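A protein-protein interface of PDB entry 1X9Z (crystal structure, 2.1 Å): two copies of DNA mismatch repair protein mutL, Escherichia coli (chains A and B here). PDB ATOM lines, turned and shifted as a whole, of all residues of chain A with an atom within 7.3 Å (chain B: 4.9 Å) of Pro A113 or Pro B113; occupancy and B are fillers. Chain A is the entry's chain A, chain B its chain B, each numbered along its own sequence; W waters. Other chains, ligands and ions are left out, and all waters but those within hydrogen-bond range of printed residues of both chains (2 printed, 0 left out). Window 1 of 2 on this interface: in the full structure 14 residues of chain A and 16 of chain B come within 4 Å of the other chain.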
ATOM      1  N   LEU A  61     -18.845 -23.842 -13.777  1.00  0.00           N
ATOM      2  CA  LEU A  61     -19.389 -23.847 -15.121  1.00  0.00           C
ATOM      3  C   LEU A  61     -20.459 -22.759 -15.240  1.00  0.00           C
ATOM      4  O   LEU A  61     -21.524 -22.871 -14.640  1.00  0.00           O
ATOM      5  CB  LEU A  61     -19.984 -25.218 -15.419  1.00  0.00           C
ATOM      6  CG  LEU A  61     -20.695 -25.349 -16.763  1.00  0.00           C
ATOM      7  CD1 LEU A  61     -19.682 -25.161 -17.913  1.00  0.00           C
ATOM      8  CD2 LEU A  61     -21.367 -26.701 -16.843  1.00  0.00           C
ATOM      9  N   LEU A  63     -23.158 -20.683 -17.461  1.00  0.00           N
ATOM     10  CA  LEU A  63     -23.958 -20.921 -18.650  1.00  0.00           C
ATOM     11  C   LEU A  63     -24.996 -19.840 -18.866  1.00  0.00           C
ATOM     12  O   LEU A  63     -25.548 -19.297 -17.908  1.00  0.00           O
ATOM     13  CB  LEU A  63     -24.696 -22.258 -18.518  1.00  0.00           C
ATOM     14  CG  LEU A  63     -23.856 -23.496 -18.235  1.00  0.00           C
ATOM     15  CD1 LEU A  63     -24.775 -24.647 -17.842  1.00  0.00           C
ATOM     16  CD2 LEU A  63     -23.030 -23.849 -19.476  1.00  0.00           C
ATOM     17  N   GLU A  69     -35.732 -20.282 -18.116  1.00  0.00           N
ATOM     18  CA  GLU A  69     -34.865 -21.320 -17.564  1.00  0.00           C
ATOM     19  C   GLU A  69     -34.332 -20.842 -16.220  1.00  0.00           C
ATOM     20  O   GLU A  69     -34.261 -21.611 -15.254  1.00  0.00           O
ATOM     21  CB  GLU A  69     -33.721 -21.627 -18.545  1.00  0.00           C
ATOM     22  CG  GLU A  69     -34.274 -22.178 -19.859  1.00  0.00           C
ATOM     23  CD  GLU A  69     -33.236 -22.453 -20.912  1.00  0.00           C
ATOM     24  OE1 GLU A  69     -32.191 -21.760 -20.947  1.00  0.00           O
ATOM     25  OE2 GLU A  69     -33.491 -23.366 -21.732  1.00  0.00           O
ATOM     26  N   ILE A  96     -22.573 -23.056 -12.019  1.00  0.00           N
ATOM     27  CA  ILE A  96     -22.599 -24.241 -11.183  1.00  0.00           C
ATOM     28  C   ILE A  96     -21.302 -24.262 -10.404  1.00  0.00           C
ATOM     29  O   ILE A  96     -20.216 -24.264 -10.992  1.00  0.00           O
ATOM     30  CB  ILE A  96     -22.692 -25.518 -12.038  1.00  0.00           C
ATOM     31  CG1 ILE A  96     -23.860 -25.402 -13.014  1.00  0.00           C
ATOM     32  CG2 ILE A  96     -22.851 -26.751 -11.132  1.00  0.00           C
ATOM     33  CD1 ILE A  96     -25.210 -25.093 -12.352  1.00  0.00           C
ATOM     34  N   ASN A 107     -19.467 -35.387 -17.829  1.00  0.00           N
ATOM     35  CA  ASN A 107     -19.143 -34.240 -18.673  1.00  0.00           C
ATOM     36  C   ASN A 107     -20.250 -33.207 -18.411  1.00  0.00           C
ATOM     37  O   ASN A 107     -21.301 -33.209 -19.066  1.00  0.00           O
ATOM     38  CB  ASN A 107     -19.121 -34.649 -20.151  1.00  0.00           C
ATOM     39  CG  ASN A 107     -18.982 -33.454 -21.080  1.00  0.00           C
ATOM     40  OD1 ASN A 107     -18.547 -32.382 -20.662  1.00  0.00           O
ATOM     41  ND2 ASN A 107     -19.347 -33.635 -22.343  1.00  0.00           N
ATOM     42  N   LEU A 108     -20.008 -32.326 -17.449  1.00  0.00           N
ATOM     43  CA  LEU A 108     -21.008 -31.339 -17.053  1.00  0.00           C
ATOM     44  C   LEU A 108     -21.415 -30.304 -18.104  1.00  0.00           C
ATOM     45  O   LEU A 108     -22.469 -29.682 -17.982  1.00  0.00           O
ATOM     46  CB  LEU A 108     -20.564 -30.645 -15.756  1.00  0.00           C
ATOM     47  CG  LEU A 108     -20.294 -31.575 -14.548  1.00  0.00           C
ATOM     48  CD1 LEU A 108     -19.829 -30.739 -13.360  1.00  0.00           C
ATOM     49  CD2 LEU A 108     -21.545 -32.357 -14.166  1.00  0.00           C
ATOM     50  N   GLN A 109     -20.600 -30.122 -19.138  1.00  0.00           N
ATOM     51  CA  GLN A 109     -20.935 -29.159 -20.191  1.00  0.00           C
ATOM     52  C   GLN A 109     -22.102 -29.649 -21.010  1.00  0.00           C
ATOM     53  O   GLN A 109     -22.725 -28.878 -21.730  1.00  0.00           O
ATOM     54  CB  GLN A 109     -19.752 -28.919 -21.113  1.00  0.00           C
ATOM     55  CG  GLN A 109     -18.582 -28.288 -20.432  1.00  0.00           C
ATOM     56  CD  GLN A 109     -17.633 -27.683 -21.426  1.00  0.00           C
ATOM     57  OE1 GLN A 109     -16.479 -27.392 -21.095  1.00  0.00           O
ATOM     58  NE2 GLN A 109     -18.113 -27.470 -22.661  1.00  0.00           N
ATOM     59  N   ILE A 110     -22.382 -30.941 -20.909  1.00  0.00           N
ATOM     60  CA  ILE A 110     -23.517 -31.529 -21.587  1.00  0.00           C
ATOM     61  C   ILE A 110     -24.597 -31.891 -20.551  1.00  0.00           C
ATOM     62  O   ILE A 110     -25.788 -31.624 -20.759  1.00  0.00           O
ATOM     63  CB  ILE A 110     -23.115 -32.815 -22.365  1.00  0.00           C
ATOM     64  CG1 ILE A 110     -22.086 -32.479 -23.460  1.00  0.00           C
ATOM     65  CG2 ILE A 110     -24.340 -33.445 -22.979  1.00  0.00           C
ATOM     66  CD1 ILE A 110     -22.580 -31.505 -24.549  1.00  0.00           C
ATOM     67  N   LEU A 111     -24.202 -32.503 -19.434  1.00  0.00           N
ATOM     68  CA  LEU A 111     -25.180 -32.886 -18.411  1.00  0.00           C
ATOM     69  C   LEU A 111     -25.961 -31.718 -17.785  1.00  0.00           C
ATOM     70  O   LEU A 111     -27.170 -31.765 -17.718  1.00  0.00           O
ATOM     71  CB  LEU A 111     -24.507 -33.705 -17.297  1.00  0.00           C
ATOM     72  CG  LEU A 111     -25.302 -33.874 -15.995  1.00  0.00           C
ATOM     73  CD1 LEU A 111     -26.400 -34.843 -16.215  1.00  0.00           C
ATOM     74  CD2 LEU A 111     -24.414 -34.392 -14.894  1.00  0.00           C
ATOM     75  N   ILE A 112     -25.281 -30.687 -17.304  1.00  0.00           N
ATOM     76  CA  ILE A 112     -25.989 -29.568 -16.683  1.00  0.00           C
ATOM     77  C   ILE A 112     -26.987 -28.867 -17.638  1.00  0.00           C
ATOM     78  O   ILE A 112     -28.142 -28.623 -17.267  1.00  0.00           O
ATOM     79  CB  ILE A 112     -24.980 -28.571 -16.076  1.00  0.00           C
ATOM     80  CG1 ILE A 112     -24.261 -29.251 -14.898  1.00  0.00           C
ATOM     81  CG2 ILE A 112     -25.690 -27.316 -15.588  1.00  0.00           C
ATOM     82  CD1 ILE A 112     -25.241 -29.823 -13.844  1.00  0.00           C
ATOM     83  N   PRO A 113     -26.560 -28.541 -18.875  1.00  0.00           N
ATOM     84  CA  PRO A 113     -27.507 -27.892 -19.788  1.00  0.00           C
ATOM     85  C   PRO A 113     -28.683 -28.841 -19.990  1.00  0.00           C
ATOM     86  O   PRO A 113     -29.818 -28.420 -20.151  1.00  0.00           O
ATOM     87  CB  PRO A 113     -26.687 -27.708 -21.066  1.00  0.00           C
ATOM     88  CG  PRO A 113     -25.335 -27.497 -20.562  1.00  0.00           C
ATOM     89  CD  PRO A 113     -25.208 -28.550 -19.460  1.00  0.00           C
ATOM     90  N   GLU A 114     -28.416 -30.141 -19.967  1.00  0.00           N
ATOM     91  CA  GLU A 114     -29.499 -31.099 -20.136  1.00  0.00           C
ATOM     92  C   GLU A 114     -30.436 -31.061 -18.937  1.00  0.00           C
ATOM     93  O   GLU A 114     -31.660 -31.118 -19.093  1.00  0.00           O
ATOM     94  CB  GLU A 114     -28.951 -32.504 -20.314  1.00  0.00           C
ATOM     95  CG  GLU A 114     -28.363 -32.792 -21.692  1.00  0.00           C
ATOM     96  CD  GLU A 114     -27.929 -34.237 -21.810  1.00  0.00           C
ATOM     97  OE1 GLU A 114     -27.009 -34.637 -21.078  1.00  0.00           O
ATOM     98  OE2 GLU A 114     -28.519 -34.980 -22.612  1.00  0.00           O
ATOM     99  N   LEU A 115     -29.862 -30.965 -17.741  1.00  0.00           N
ATOM    100  CA  LEU A 115     -30.655 -30.896 -16.521  1.00  0.00           C
ATOM    101  C   LEU A 115     -31.479 -29.606 -16.567  1.00  0.00           C
ATOM    102  O   LEU A 115     -32.671 -29.606 -16.238  1.00  0.00           O
ATOM    103  CB  LEU A 115     -29.736 -30.878 -15.299  1.00  0.00           C
ATOM    104  CG  LEU A 115     -30.391 -30.733 -13.920  1.00  0.00           C
ATOM    105  CD1 LEU A 115     -31.336 -31.895 -13.673  1.00  0.00           C
ATOM    106  CD2 LEU A 115     -29.309 -30.706 -12.851  1.00  0.00           C
ATOM    107  N   ILE A 116     -30.844 -28.515 -16.985  1.00  0.00           N
ATOM    108  CA  ILE A 116     -31.533 -27.230 -17.091  1.00  0.00           C
ATOM    109  C   ILE A 116     -32.743 -27.338 -18.023  1.00  0.00           C
ATOM    110  O   ILE A 116     -33.804 -26.801 -17.718  1.00  0.00           O
ATOM    111  CB  ILE A 116     -30.562 -26.093 -17.584  1.00  0.00           C
ATOM    112  CG1 ILE A 116     -29.540 -25.763 -16.491  1.00  0.00           C
ATOM    113  CG2 ILE A 116     -31.341 -24.820 -17.907  1.00  0.00           C
ATOM    114  CD1 ILE A 116     -28.415 -24.816 -16.934  1.00  0.00           C
ATOM    115  N   GLY A 117     -32.588 -28.037 -19.149  1.00  0.00           N
ATOM    116  CA  GLY A 117     -33.698 -28.213 -20.080  1.00  0.00           C
ATOM    117  C   GLY A 117     -34.834 -29.006 -19.445  1.00  0.00           C
ATOM    118  O   GLY A 117     -36.015 -28.694 -19.625  1.00  0.00           O
ATOM    119  N   TYR A 118     -34.483 -30.041 -18.692  1.00  0.00           N
ATOM    120  CA  TYR A 118     -35.484 -30.861 -18.019  1.00  0.00           C
ATOM    121  C   TYR A 118     -36.243 -30.017 -16.985  1.00  0.00           C
ATOM    122  O   TYR A 118     -37.470 -30.070 -16.912  1.00  0.00           O
ATOM    123  CB  TYR A 118     -34.804 -32.041 -17.318  1.00  0.00           C
ATOM    124  CG  TYR A 118     -35.700 -32.792 -16.365  1.00  0.00           C
ATOM    125  CD1 TYR A 118     -36.652 -33.687 -16.834  1.00  0.00           C
ATOM    126  CD2 TYR A 118     -35.626 -32.575 -14.994  1.00  0.00           C
ATOM    127  CE1 TYR A 118     -37.508 -34.349 -15.966  1.00  0.00           C
ATOM    128  CE2 TYR A 118     -36.478 -33.232 -14.118  1.00  0.00           C
ATOM    129  CZ  TYR A 118     -37.416 -34.121 -14.619  1.00  0.00           C
ATOM    130  OH  TYR A 118     -38.261 -34.798 -13.761  1.00  0.00           O
ATOM    131  N   LEU A 119     -35.498 -29.242 -16.198  1.00  0.00           N
ATOM    132  CA  LEU A 119     -36.060 -28.391 -15.153  1.00  0.00           C
ATOM    133  C   LEU A 119     -36.998 -27.315 -15.685  1.00  0.00           C
ATOM    134  O   LEU A 119     -38.008 -26.993 -15.055  1.00  0.00           O
ATOM    135  CB  LEU A 119     -34.935 -27.712 -14.359  1.00  0.00           C
ATOM    136  CG  LEU A 119     -34.012 -28.601 -13.522  1.00  0.00           C
ATOM    137  CD1 LEU A 119     -32.962 -27.749 -12.833  1.00  0.00           C
ATOM    138  CD2 LEU A 119     -34.835 -29.360 -12.491  1.00  0.00           C
ATOM    139  N   LEU A 138     -29.455 -38.590 -18.241  1.00  0.00           N
ATOM    140  CA  LEU A 138     -28.274 -37.779 -18.450  1.00  0.00           C
ATOM    141  C   LEU A 138     -26.902 -38.346 -18.229  1.00  0.00           C
ATOM    142  O   LEU A 138     -25.911 -37.689 -18.560  1.00  0.00           O
ATOM    143  CB  LEU A 138     -28.384 -36.509 -17.612  1.00  0.00           C
ATOM    144  CG  LEU A 138     -29.614 -35.636 -17.832  1.00  0.00           C
ATOM    145  CD1 LEU A 138     -29.496 -34.328 -17.040  1.00  0.00           C
ATOM    146  CD2 LEU A 138     -29.747 -35.368 -19.320  1.00  0.00           C
ATOM    147  N   LEU B  63     -18.425 -26.838 -27.580  1.00  0.00           N
ATOM    148  CA  LEU B  63     -18.819 -27.652 -26.439  1.00  0.00           C
ATOM    149  C   LEU B  63     -17.871 -28.810 -26.237  1.00  0.00           C
ATOM    150  O   LEU B  63     -17.438 -29.450 -27.201  1.00  0.00           O
ATOM    151  CB  LEU B  63     -20.223 -28.220 -26.660  1.00  0.00           C
ATOM    152  CG  LEU B  63     -21.390 -27.249 -26.872  1.00  0.00           C
ATOM    153  CD1 LEU B  63     -22.566 -27.991 -27.505  1.00  0.00           C
ATOM    154  CD2 LEU B  63     -21.776 -26.651 -25.526  1.00  0.00           C
ATOM    155  N   LEU B 108     -29.823 -22.645 -28.044  1.00  0.00           N
ATOM    156  CA  LEU B 108     -28.876 -23.651 -28.490  1.00  0.00           C
ATOM    157  C   LEU B 108     -27.908 -24.125 -27.407  1.00  0.00           C
ATOM    158  O   LEU B 108     -27.416 -25.245 -27.491  1.00  0.00           O
ATOM    159  CB  LEU B 108     -28.104 -23.127 -29.706  1.00  0.00           C
ATOM    160  CG  LEU B 108     -29.017 -22.745 -30.885  1.00  0.00           C
ATOM    161  CD1 LEU B 108     -28.179 -22.257 -32.049  1.00  0.00           C
ATOM    162  CD2 LEU B 108     -29.860 -23.956 -31.311  1.00  0.00           C
ATOM    163  N   GLN B 109     -27.647 -23.294 -26.392  1.00  0.00           N
ATOM    164  CA  GLN B 109     -26.717 -23.681 -25.328  1.00  0.00           C
ATOM    165  C   GLN B 109     -27.338 -24.788 -24.493  1.00  0.00           C
ATOM    166  O   GLN B 109     -26.656 -25.414 -23.689  1.00  0.00           O
ATOM    167  CB  GLN B 109     -26.360 -22.498 -24.396  1.00  0.00           C
ATOM    168  CG  GLN B 109     -26.837 -21.111 -24.846  1.00  0.00           C
ATOM    169  CD  GLN B 109     -28.312 -20.833 -24.527  1.00  0.00           C
ATOM    170  OE1 GLN B 109     -28.664 -20.390 -23.424  1.00  0.00           O
ATOM    171  NE2 GLN B 109     -29.179 -21.099 -25.497  1.00  0.00           N
ATOM    172  N   ILE B 110     -28.635 -25.004 -24.683  1.00  0.00           N
ATOM    173  CA  ILE B 110     -29.377 -26.034 -23.974  1.00  0.00           C
ATOM    174  C   ILE B 110     -29.817 -27.153 -24.940  1.00  0.00           C
ATOM    175  O   ILE B 110     -29.632 -28.339 -24.672  1.00  0.00           O
ATOM    176  CB  ILE B 110     -30.623 -25.430 -23.290  1.00  0.00           C
ATOM    177  CG1 ILE B 110     -30.204 -24.456 -22.188  1.00  0.00           C
ATOM    178  CG2 ILE B 110     -31.489 -26.526 -22.702  1.00  0.00           C
ATOM    179  CD1 ILE B 110     -29.412 -25.106 -21.057  1.00  0.00           C
ATOM    180  N   LEU B 111     -30.396 -26.763 -26.064  1.00  0.00           N
ATOM    181  CA  LEU B 111     -30.879 -27.710 -27.066  1.00  0.00           C
ATOM    182  C   LEU B 111     -29.793 -28.583 -27.729  1.00  0.00           C
ATOM    183  O   LEU B 111     -29.998 -29.778 -27.934  1.00  0.00           O
ATOM    184  CB  LEU B 111     -31.665 -26.944 -28.143  1.00  0.00           C
ATOM    185  CG  LEU B 111     -32.213 -27.800 -29.275  1.00  0.00           C
ATOM    186  CD1 LEU B 111     -33.259 -28.750 -28.703  1.00  0.00           C
ATOM    187  CD2 LEU B 111     -32.802 -26.921 -30.368  1.00  0.00           C
ATOM    188  N   ILE B 112     -28.644 -28.011 -28.076  1.00  0.00           N
ATOM    189  CA  ILE B 112     -27.591 -28.824 -28.702  1.00  0.00           C
ATOM    190  C   ILE B 112     -27.081 -29.886 -27.714  1.00  0.00           C
ATOM    191  O   ILE B 112     -26.971 -31.065 -28.061  1.00  0.00           O
ATOM    192  CB  ILE B 112     -26.460 -27.935 -29.236  1.00  0.00           C
ATOM    193  CG1 ILE B 112     -27.020 -27.080 -30.379  1.00  0.00           C
ATOM    194  CG2 ILE B 112     -25.311 -28.794 -29.788  1.00  0.00           C
ATOM    195  CD1 ILE B 112     -27.565 -27.956 -31.548  1.00  0.00           C
ATOM    196  N   PRO B 113     -26.755 -29.482 -26.474  1.00  0.00           N
ATOM    197  CA  PRO B 113     -26.293 -30.469 -25.491  1.00  0.00           C
ATOM    198  C   PRO B 113     -27.325 -31.602 -25.355  1.00  0.00           C
ATOM    199  O   PRO B 113     -26.957 -32.782 -25.260  1.00  0.00           O
ATOM    200  CB  PRO B 113     -26.154 -29.632 -24.211  1.00  0.00           C
ATOM    201  CG  PRO B 113     -25.611 -28.340 -24.756  1.00  0.00           C
ATOM    202  CD  PRO B 113     -26.459 -28.107 -26.016  1.00  0.00           C
ATOM    203  N   GLU B 114     -28.613 -31.252 -25.342  1.00  0.00           N
ATOM    204  CA  GLU B 114     -29.683 -32.261 -25.266  1.00  0.00           C
ATOM    205  C   GLU B 114     -29.640 -33.167 -26.501  1.00  0.00           C
ATOM    206  O   GLU B 114     -29.820 -34.390 -26.396  1.00  0.00           O
ATOM    207  CB  GLU B 114     -31.070 -31.599 -25.181  1.00  0.00           C
ATOM    208  CG  GLU B 114     -31.298 -30.757 -23.919  1.00  0.00           C
ATOM    209  CD  GLU B 114     -32.662 -30.110 -23.882  1.00  0.00           C
ATOM    210  OE1 GLU B 114     -33.079 -29.541 -24.916  1.00  0.00           O
ATOM    211  OE2 GLU B 114     -33.312 -30.151 -22.818  1.00  0.00           O
ATOM    212  N   LEU B 115     -29.414 -32.572 -27.670  1.00  0.00           N
ATOM    213  CA  LEU B 115     -29.325 -33.343 -28.920  1.00  0.00           C
ATOM    214  C   LEU B 115     -28.110 -34.286 -28.813  1.00  0.00           C
ATOM    215  O   LEU B 115     -28.182 -35.462 -29.151  1.00  0.00           O
ATOM    216  CB  LEU B 115     -29.144 -32.396 -30.129  1.00  0.00           C
ATOM    217  CG  LEU B 115     -28.853 -33.064 -31.485  1.00  0.00           C
ATOM    218  CD1 LEU B 115     -30.065 -33.894 -31.930  1.00  0.00           C
ATOM    219  CD2 LEU B 115     -28.540 -31.998 -32.528  1.00  0.00           C
ATOM    220  N   ILE B 116     -26.998 -33.758 -28.311  1.00  0.00           N
ATOM    221  CA  ILE B 116     -25.799 -34.568 -28.163  1.00  0.00           C
ATOM    222  C   ILE B 116     -26.081 -35.744 -27.212  1.00  0.00           C
ATOM    223  O   ILE B 116     -25.717 -36.888 -27.494  1.00  0.00           O
ATOM    224  CB  ILE B 116     -24.630 -33.685 -27.662  1.00  0.00           C
ATOM    225  CG1 ILE B 116     -24.175 -32.758 -28.800  1.00  0.00           C
ATOM    226  CG2 ILE B 116     -23.477 -34.547 -27.177  1.00  0.00           C
ATOM    227  CD1 ILE B 116     -23.165 -31.650 -28.354  1.00  0.00           C
ATOM    228  N   GLY B 117     -26.760 -35.465 -26.102  1.00  0.00           N
ATOM    229  CA  GLY B 117     -27.093 -36.516 -25.157  1.00  0.00           C
ATOM    230  C   GLY B 117     -27.967 -37.558 -25.831  1.00  0.00           C
ATOM    231  O   GLY B 117     -27.803 -38.773 -25.636  1.00  0.00           O
HETATM  232  O   HOH W   1     -33.052 -32.617 -20.709  1.00  0.00           O
HETATM  233  O   HOH W   2     -31.157 -35.620 -24.343  1.00  0.00           O
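Ile B110 touches Glu A69 (CG1 to OE2, 3.5 Å).
Gln A109 touches Leu B63.
Pro B113 touches Ile A110.
CD1 of Ile B116 touches CD1 of Ile A110, at 3.9 Å.
Pro A113 touches Gln B109 (CB to O, 3.5 Å).
Pro A113 touches Ile B110.
OE2 of Glu A114 touches O of Pro B113 (3.8 Å).
CG of Glu A114 touches CA of Glu B114 (3.8 Å).
CD1 of Ile B110 touches CG2 of Ile A116, 3.7 Å away.
Gly A117 touches Ile B110 (CA to CG2, 3.8 Å).
Water W1 lies within hydrogen-bond range of the backbone carbonyl oxygen (O) of Glu A114 (2.6 Å) and the side-chain carboxylate (OE2) of Glu B114 (3.3 Å).
Water W2 bridges O of Glu B114 and OE2 of Glu A114.
Printed residues of chain B that touch a printed residue of chain A: Leu B63, Gln B109, Ile B110, Pro B113, Glu B114, Ile B116 and Gly B117.
Hydrophobic or aromatic side chains of chain B that line the printed part of chain A: Ile B110, Pro B113 and Ile B116.
Along chain B the printed residues that touch a printed residue of chain A span positions 63 to 117.
Printed residues of chain A that touch a printed residue of chain B: Glu A69, Gln A109, Ile A110, Pro A113, Glu A114, Ile A116 and Gly A117.
Hydrophobic or aromatic side chains of chain A that line the printed part of chain B: Ile A110, Pro A113 and Ile A116.
Among the printed residues, no Asp or Glu carboxylate lies within 4 Å of a Lys or Arg side-chain nitrogen of the other chain.
Ile A110 touches Pro B113, and with the chains exchanged Pro A113 touches Ile B110.
Glu A114 touches Pro B113, but with the chains exchanged Pro A113 does not touch Glu B114 (4.7 Å).
Glu A114 touches its own counterpart, Glu B114.
Gly A117 touches Ile B110, but with the chains exchanged Ile A110 does not touch Gly B117 (4.4 Å).
Of the 13 pairs that touch across the chains among the printed residues, 8 have their exchanged pair printed and touching as well.
The backbone NH of Gln A109 sits close to the side-chain amide oxygen of Asn A107 (3.4 Å).
Pro A113 touches just these residues of chain B: Gln B109, Ile B110 and Pro B113.
Of the printed residues of chain A, Pro B113 touches Ile A110, Pro A113 and Glu A114.
Of the printed residues of chain A, Leu B63 touches Gln A109 (3.8 Å).
Printed residues of chain B within 4 Å of Glu A69: Ile B110 (3.5 Å).
Printed residues of chain B within 4 Å of Ile A110: Pro B113 and Ile B116.
Printed residues of chain B within 4 Å of Ile A116: Ile B110 (3.7 Å).
Of the printed residues of chain B, Gln A109 touches Leu B63 (3.8 Å).
Leu A119 touches none of the printed residues of chain B.
The nearest printed residue of chain B that does not touch Glu A69 is Gln B109 (4.5 Å).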
